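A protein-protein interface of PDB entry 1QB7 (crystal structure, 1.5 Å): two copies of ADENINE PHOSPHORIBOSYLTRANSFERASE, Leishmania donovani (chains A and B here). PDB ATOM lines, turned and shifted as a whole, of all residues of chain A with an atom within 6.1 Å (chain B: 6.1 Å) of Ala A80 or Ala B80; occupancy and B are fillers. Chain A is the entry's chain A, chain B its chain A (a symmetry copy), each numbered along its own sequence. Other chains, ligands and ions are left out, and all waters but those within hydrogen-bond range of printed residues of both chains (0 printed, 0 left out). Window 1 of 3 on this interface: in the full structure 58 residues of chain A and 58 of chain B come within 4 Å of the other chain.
The guanidinium group (NE) of Arg A101 lies within salt-bridge range of the side-chain carboxylate (OD2) of Asp A79. The guanidinium group (NE) of Arg B101 is in salt-bridge range of the side-chain carboxylate (OD2) of Asp B79 (2.7 Å).
Printed residues of chain B that touch a printed residue of chain A: Asp B79, Ala B80, Arg B81, Phe B83, Leu B84 and Arg B101. Hydrophobic or aromatic side chains of chain B that line the printed part of chain A: Ala B80, Phe B83 and Leu B84. Among the printed residues, no Asp or Glu carboxylate lies within 4 Å of a Lys or Arg side-chain nitrogen of the other chain.
Asp A79 touches Ala B80, and with the chains exchanged Ala A80 touches Asp B79. Ala B80 touches its own counterpart, Ala A80. Ala A80 touches Arg B101, and with the chains exchanged Arg A101 touches Ala B80. Phe B83 touches its own counterpart, Phe A83. Positions printed for both chains: 78, 79, 80, 81, 82, 83, 84, 101 and 145. Of the 12 pairs that touch across the chains among the printed residues, 12 have their exchanged pair printed and touching as well.
Printed residues of chain B within 4 Å of Ala A80: Asp B79 (3.5 Å), Ala B80 (3.5 Å), Phe B83 (3.7 Å) and Arg B101 (3.7 Å). Of the printed residues of chain B, Arg A81 touches Arg B101 (3.8 Å). Of the printed residues of chain B, Arg A101 touches Ala B80 and Arg B81. Printed residues of chain A within 4 Å of Ala B80: Asp A79, Ala A80, Phe A83 and Arg A101. Printed residues of chain A within 4 Å of Phe B83: Ala A80, Phe A83 and Leu A84. Of the printed residues of chain A, Leu B84 touches Phe A83. The nearest printed residue of chain A that does not touch Ala B80 is Arg A81 (6.6 Å).
The backbone carbonyl oxygen of Phe B83 sits close to the backbone carbonyl oxygen of Phe A83 (3.1 Å).
Among the printed residues, pairs that only touch across the chains: Asp A79 with Ala B80, Ala A80 with Asp B79, Ala A80 with Ala B80, Ala A80 with Phe B83, Ala A80 with Arg B101, Arg A81 with Arg B101, Phe A83 with Ala B80, Phe A83 with Leu B84, Leu A84 with Phe B83, Arg A101 with Ala B80 and Arg A101 with Arg B81.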
ATOM      1  N   PHE A  78     -24.672  -8.490   3.019  1.00  0.00           N
ATOM      2  CA  PHE A  78     -25.236  -9.813   3.286  1.00  0.00           C
ATOM      3  C   PHE A  78     -24.435 -10.934   2.620  1.00  0.00           C
ATOM      4  O   PHE A  78     -24.033 -10.824   1.464  1.00  0.00           O
ATOM      5  CB  PHE A  78     -26.693  -9.881   2.802  1.00  0.00           C
ATOM      6  CG  PHE A  78     -27.610  -8.848   3.422  1.00  0.00           C
ATOM      7  CD1 PHE A  78     -27.144  -7.933   4.361  1.00  0.00           C
ATOM      8  CD2 PHE A  78     -28.947  -8.785   3.039  1.00  0.00           C
ATOM      9  CE1 PHE A  78     -27.998  -6.969   4.907  1.00  0.00           C
ATOM     10  CE2 PHE A  78     -29.807  -7.829   3.575  1.00  0.00           C
ATOM     11  CZ  PHE A  78     -29.331  -6.919   4.510  1.00  0.00           C
ATOM     12  N   ASP A  79     -24.236 -12.023   3.362  1.00  0.00           N
ATOM     13  CA  ASP A  79     -23.495 -13.195   2.886  1.00  0.00           C
ATOM     14  C   ASP A  79     -24.346 -13.926   1.838  1.00  0.00           C
ATOM     15  O   ASP A  79     -25.486 -14.280   2.125  1.00  0.00           O
ATOM     16  CB  ASP A  79     -23.224 -14.108   4.089  1.00  0.00           C
ATOM     17  CG  ASP A  79     -22.315 -15.289   3.769  1.00  0.00           C
ATOM     18  OD1 ASP A  79     -21.884 -15.470   2.618  1.00  0.00           O
ATOM     19  OD2 ASP A  79     -22.012 -16.049   4.705  1.00  0.00           O
ATOM     20  N   ALA A  80     -23.832 -14.128   0.621  1.00  0.00           N
ATOM     21  CA  ALA A  80     -22.490 -13.717   0.198  1.00  0.00           C
ATOM     22  C   ALA A  80     -22.500 -12.687  -0.929  1.00  0.00           C
ATOM     23  O   ALA A  80     -21.490 -12.044  -1.193  1.00  0.00           O
ATOM     24  CB  ALA A  80     -21.702 -14.941  -0.265  1.00  0.00           C
ATOM     25  N   ARG A  81     -23.635 -12.528  -1.594  1.00  0.00           N
ATOM     26  CA  ARG A  81     -23.703 -11.613  -2.720  1.00  0.00           C
ATOM     27  C   ARG A  81     -23.522 -10.133  -2.381  1.00  0.00           C
ATOM     28  O   ARG A  81     -23.077  -9.351  -3.227  1.00  0.00           O
ATOM     29  CB  ARG A  81     -24.950 -11.918  -3.553  1.00  0.00           C
ATOM     30  CG  ARG A  81     -25.009 -13.412  -3.909  1.00  0.00           C
ATOM     31  CD  ARG A  81     -26.106 -13.789  -4.882  1.00  0.00           C
ATOM     32  NE  ARG A  81     -27.433 -13.383  -4.436  1.00  0.00           N
ATOM     33  CZ  ARG A  81     -28.514 -14.159  -4.464  1.00  0.00           C
ATOM     34  NH1 ARG A  81     -28.430 -15.419  -4.863  1.00  0.00           N
ATOM     35  NH2 ARG A  81     -29.679 -13.685  -4.051  1.00  0.00           N
ATOM     36  N   GLY A  82     -23.798  -9.771  -1.127  1.00  0.00           N
ATOM     37  CA  GLY A  82     -23.608  -8.399  -0.682  1.00  0.00           C
ATOM     38  C   GLY A  82     -22.117  -8.122  -0.493  1.00  0.00           C
ATOM     39  O   GLY A  82     -21.676  -6.968  -0.516  1.00  0.00           O
ATOM     40  N   PHE A  83     -21.344  -9.192  -0.300  1.00  0.00           N
ATOM     41  CA  PHE A  83     -19.891  -9.110  -0.125  1.00  0.00           C
ATOM     42  C   PHE A  83     -19.227  -8.674  -1.428  1.00  0.00           C
ATOM     43  O   PHE A  83     -18.105  -8.173  -1.430  1.00  0.00           O
ATOM     44  CB  PHE A  83     -19.315 -10.483   0.244  1.00  0.00           C
ATOM     45  CG  PHE A  83     -19.668 -10.962   1.627  1.00  0.00           C
ATOM     46  CD1 PHE A  83     -20.568 -10.265   2.432  1.00  0.00           C
ATOM     47  CD2 PHE A  83     -19.075 -12.117   2.134  1.00  0.00           C
ATOM     48  CE1 PHE A  83     -20.872 -10.716   3.722  1.00  0.00           C
ATOM     49  CE2 PHE A  83     -19.371 -12.572   3.415  1.00  0.00           C
ATOM     50  CZ  PHE A  83     -20.272 -11.869   4.213  1.00  0.00           C
ATOM     51  N   LEU A  84     -19.925  -8.897  -2.534  1.00  0.00           N
ATOM     52  CA  LEU A  84     -19.427  -8.568  -3.860  1.00  0.00           C
ATOM     53  C   LEU A  84     -19.416  -7.086  -4.188  1.00  0.00           C
ATOM     54  O   LEU A  84     -18.630  -6.645  -5.025  1.00  0.00           O
ATOM     55  CB  LEU A  84     -20.261  -9.298  -4.918  1.00  0.00           C
ATOM     56  CG  LEU A  84     -20.250 -10.828  -4.863  1.00  0.00           C
ATOM     57  CD1 LEU A  84     -21.362 -11.378  -5.734  1.00  0.00           C
ATOM     58  CD2 LEU A  84     -18.901 -11.351  -5.315  1.00  0.00           C
ATOM     59  N   ARG A 101     -23.613 -12.669   8.536  1.00  0.00           N
ATOM     60  CA  ARG A 101     -23.550 -14.079   8.171  1.00  0.00           C
ATOM     61  C   ARG A 101     -24.258 -14.946   9.204  1.00  0.00           C
ATOM     62  O   ARG A 101     -24.624 -14.471  10.278  1.00  0.00           O
ATOM     63  CB  ARG A 101     -22.090 -14.539   8.094  1.00  0.00           C
ATOM     64  CG  ARG A 101     -21.103 -13.533   7.499  1.00  0.00           C
ATOM     65  CD  ARG A 101     -19.753 -14.187   7.246  1.00  0.00           C
ATOM     66  NE  ARG A 101     -19.885 -15.227   6.235  1.00  0.00           N
ATOM     67  CZ  ARG A 101     -18.888 -15.965   5.760  1.00  0.00           C
ATOM     68  NH1 ARG A 101     -17.652 -15.803   6.210  1.00  0.00           N
ATOM     69  NH2 ARG A 101     -19.139 -16.881   4.838  1.00  0.00           N
ATOM     70  N   ASP A 145     -27.038  -5.803  -0.578  1.00  0.00           N
ATOM     71  CA  ASP A 145     -27.175  -7.168  -1.083  1.00  0.00           C
ATOM     72  C   ASP A 145     -27.473  -6.980  -2.575  1.00  0.00           C
ATOM     73  O   ASP A 145     -27.776  -5.868  -3.011  1.00  0.00           O
ATOM     74  CB  ASP A 145     -28.343  -7.878  -0.380  1.00  0.00           C
ATOM     75  CG  ASP A 145     -28.315  -9.398  -0.549  1.00  0.00           C
ATOM     76  OD1 ASP A 145     -27.330  -9.953  -1.087  1.00  0.00           O
ATOM     77  OD2 ASP A 145     -29.289 -10.042  -0.117  1.00  0.00           O
ATOM     78  N   PHE B  78     -13.161 -17.238  -4.057  1.00  0.00           N
ATOM     79  CA  PHE B  78     -13.836 -18.329  -3.357  1.00  0.00           C
ATOM     80  C   PHE B  78     -14.958 -17.830  -2.442  1.00  0.00           C
ATOM     81  O   PHE B  78     -14.797 -16.845  -1.724  1.00  0.00           O
ATOM     82  CB  PHE B  78     -12.829 -19.136  -2.522  1.00  0.00           C
ATOM     83  CG  PHE B  78     -11.686 -19.728  -3.319  1.00  0.00           C
ATOM     84  CD1 PHE B  78     -11.590 -19.551  -4.695  1.00  0.00           C
ATOM     85  CD2 PHE B  78     -10.688 -20.451  -2.672  1.00  0.00           C
ATOM     86  CE1 PHE B  78     -10.515 -20.084  -5.415  1.00  0.00           C
ATOM     87  CE2 PHE B  78      -9.612 -20.986  -3.376  1.00  0.00           C
ATOM     88  CZ  PHE B  78      -9.525 -20.801  -4.750  1.00  0.00           C
ATOM     89  N   ASP B  79     -16.082 -18.543  -2.461  1.00  0.00           N
ATOM     90  CA  ASP B  79     -17.257 -18.216  -1.648  1.00  0.00           C
ATOM     91  C   ASP B  79     -16.945 -18.535  -0.179  1.00  0.00           C
ATOM     92  O   ASP B  79     -16.567 -19.662   0.127  1.00  0.00           O
ATOM     93  CB  ASP B  79     -18.434 -19.066  -2.145  1.00  0.00           C
ATOM     94  CG  ASP B  79     -19.765 -18.708  -1.494  1.00  0.00           C
ATOM     95  OD1 ASP B  79     -19.834 -17.822  -0.626  1.00  0.00           O
ATOM     96  OD2 ASP B  79     -20.774 -19.322  -1.881  1.00  0.00           O
ATOM     97  N   ALA B  80     -17.064 -17.561   0.729  1.00  0.00           N
ATOM     98  CA  ALA B  80     -17.489 -16.190   0.438  1.00  0.00           C
ATOM     99  C   ALA B  80     -16.415 -15.147   0.735  1.00  0.00           C
ATOM    100  O   ALA B  80     -16.510 -14.009   0.285  1.00  0.00           O
ATOM    101  CB  ALA B  80     -18.734 -15.855   1.257  1.00  0.00           C
ATOM    102  N   ARG B  81     -15.393 -15.527   1.488  1.00  0.00           N
ATOM    103  CA  ARG B  81     -14.365 -14.572   1.866  1.00  0.00           C
ATOM    104  C   ARG B  81     -13.510 -14.035   0.718  1.00  0.00           C
ATOM    105  O   ARG B  81     -12.981 -12.922   0.805  1.00  0.00           O
ATOM    106  CB  ARG B  81     -13.559 -15.127   3.042  1.00  0.00           C
ATOM    107  CG  ARG B  81     -14.497 -15.574   4.176  1.00  0.00           C
ATOM    108  CD  ARG B  81     -13.798 -15.970   5.458  1.00  0.00           C
ATOM    109  NE  ARG B  81     -12.798 -17.013   5.268  1.00  0.00           N
ATOM    110  CZ  ARG B  81     -12.669 -18.092   6.039  1.00  0.00           C
ATOM    111  NH1 ARG B  81     -13.516 -18.316   7.032  1.00  0.00           N
ATOM    112  NH2 ARG B  81     -11.713 -18.972   5.788  1.00  0.00           N
ATOM    113  N   GLY B  82     -13.436 -14.793  -0.377  1.00  0.00           N
ATOM    114  CA  GLY B  82     -12.696 -14.351  -1.549  1.00  0.00           C
ATOM    115  C   GLY B  82     -13.489 -13.270  -2.281  1.00  0.00           C
ATOM    116  O   GLY B  82     -12.927 -12.473  -3.040  1.00  0.00           O
ATOM    117  N   PHE B  83     -14.803 -13.253  -2.053  1.00  0.00           N
ATOM    118  CA  PHE B  83     -15.709 -12.271  -2.654  1.00  0.00           C
ATOM    119  C   PHE B  83     -15.436 -10.883  -2.082  1.00  0.00           C
ATOM    120  O   PHE B  83     -15.780  -9.870  -2.686  1.00  0.00           O
ATOM    121  CB  PHE B  83     -17.169 -12.618  -2.334  1.00  0.00           C
ATOM    122  CG  PHE B  83     -17.692 -13.844  -3.034  1.00  0.00           C
ATOM    123  CD1 PHE B  83     -16.854 -14.665  -3.790  1.00  0.00           C
ATOM    124  CD2 PHE B  83     -19.045 -14.169  -2.948  1.00  0.00           C
ATOM    125  CE1 PHE B  83     -17.361 -15.792  -4.447  1.00  0.00           C
ATOM    126  CE2 PHE B  83     -19.557 -15.286  -3.599  1.00  0.00           C
ATOM    127  CZ  PHE B  83     -18.712 -16.101  -4.352  1.00  0.00           C
ATOM    128  N   LEU B  84     -14.838 -10.854  -0.897  1.00  0.00           N
ATOM    129  CA  LEU B  84     -14.532  -9.616  -0.200  1.00  0.00           C
ATOM    130  C   LEU B  84     -13.374  -8.825  -0.783  1.00  0.00           C
ATOM    131  O   LEU B  84     -13.309  -7.609  -0.609  1.00  0.00           O
ATOM    132  CB  LEU B  84     -14.227  -9.918   1.272  1.00  0.00           C
ATOM    133  CG  LEU B  84     -15.353 -10.560   2.086  1.00  0.00           C
ATOM    134  CD1 LEU B  84     -14.799 -11.095   3.392  1.00  0.00           C
ATOM    135  CD2 LEU B  84     -16.449  -9.543   2.341  1.00  0.00           C
ATOM    136  N   ARG B 101     -18.435 -21.266  -6.286  1.00  0.00           N
ATOM    137  CA  ARG B 101     -19.386 -21.585  -5.229  1.00  0.00           C
ATOM    138  C   ARG B 101     -19.865 -23.027  -5.337  1.00  0.00           C
ATOM    139  O   ARG B 101     -19.602 -23.704  -6.331  1.00  0.00           O
ATOM    140  CB  ARG B 101     -20.615 -20.675  -5.332  1.00  0.00           C
ATOM    141  CG  ARG B 101     -20.340 -19.221  -5.722  1.00  0.00           C
ATOM    142  CD  ARG B 101     -21.588 -18.370  -5.548  1.00  0.00           C
ATOM    143  NE  ARG B 101     -21.963 -18.316  -4.142  1.00  0.00           N
ATOM    144  CZ  ARG B 101     -22.985 -17.629  -3.647  1.00  0.00           C
ATOM    145  NH1 ARG B 101     -23.776 -16.926  -4.444  1.00  0.00           N
ATOM    146  NH2 ARG B 101     -23.222 -17.661  -2.345  1.00  0.00           N
ATOM    147  N   ASP B 145      -8.694 -15.834  -2.098  1.00  0.00           N
ATOM    148  CA  ASP B 145      -9.446 -16.201  -0.899  1.00  0.00           C
ATOM    149  C   ASP B 145      -8.693 -15.501   0.237  1.00  0.00           C
ATOM    150  O   ASP B 145      -7.573 -15.025   0.036  1.00  0.00           O
ATOM    151  CB  ASP B 145      -9.427 -17.726  -0.708  1.00  0.00           C
ATOM    152  CG  ASP B 145     -10.492 -18.225   0.271  1.00  0.00           C
ATOM    153  OD1 ASP B 145     -11.357 -17.437   0.715  1.00  0.00           O
ATOM    154  OD2 ASP B 145     -10.468 -19.431   0.579  1.00  0.00           O
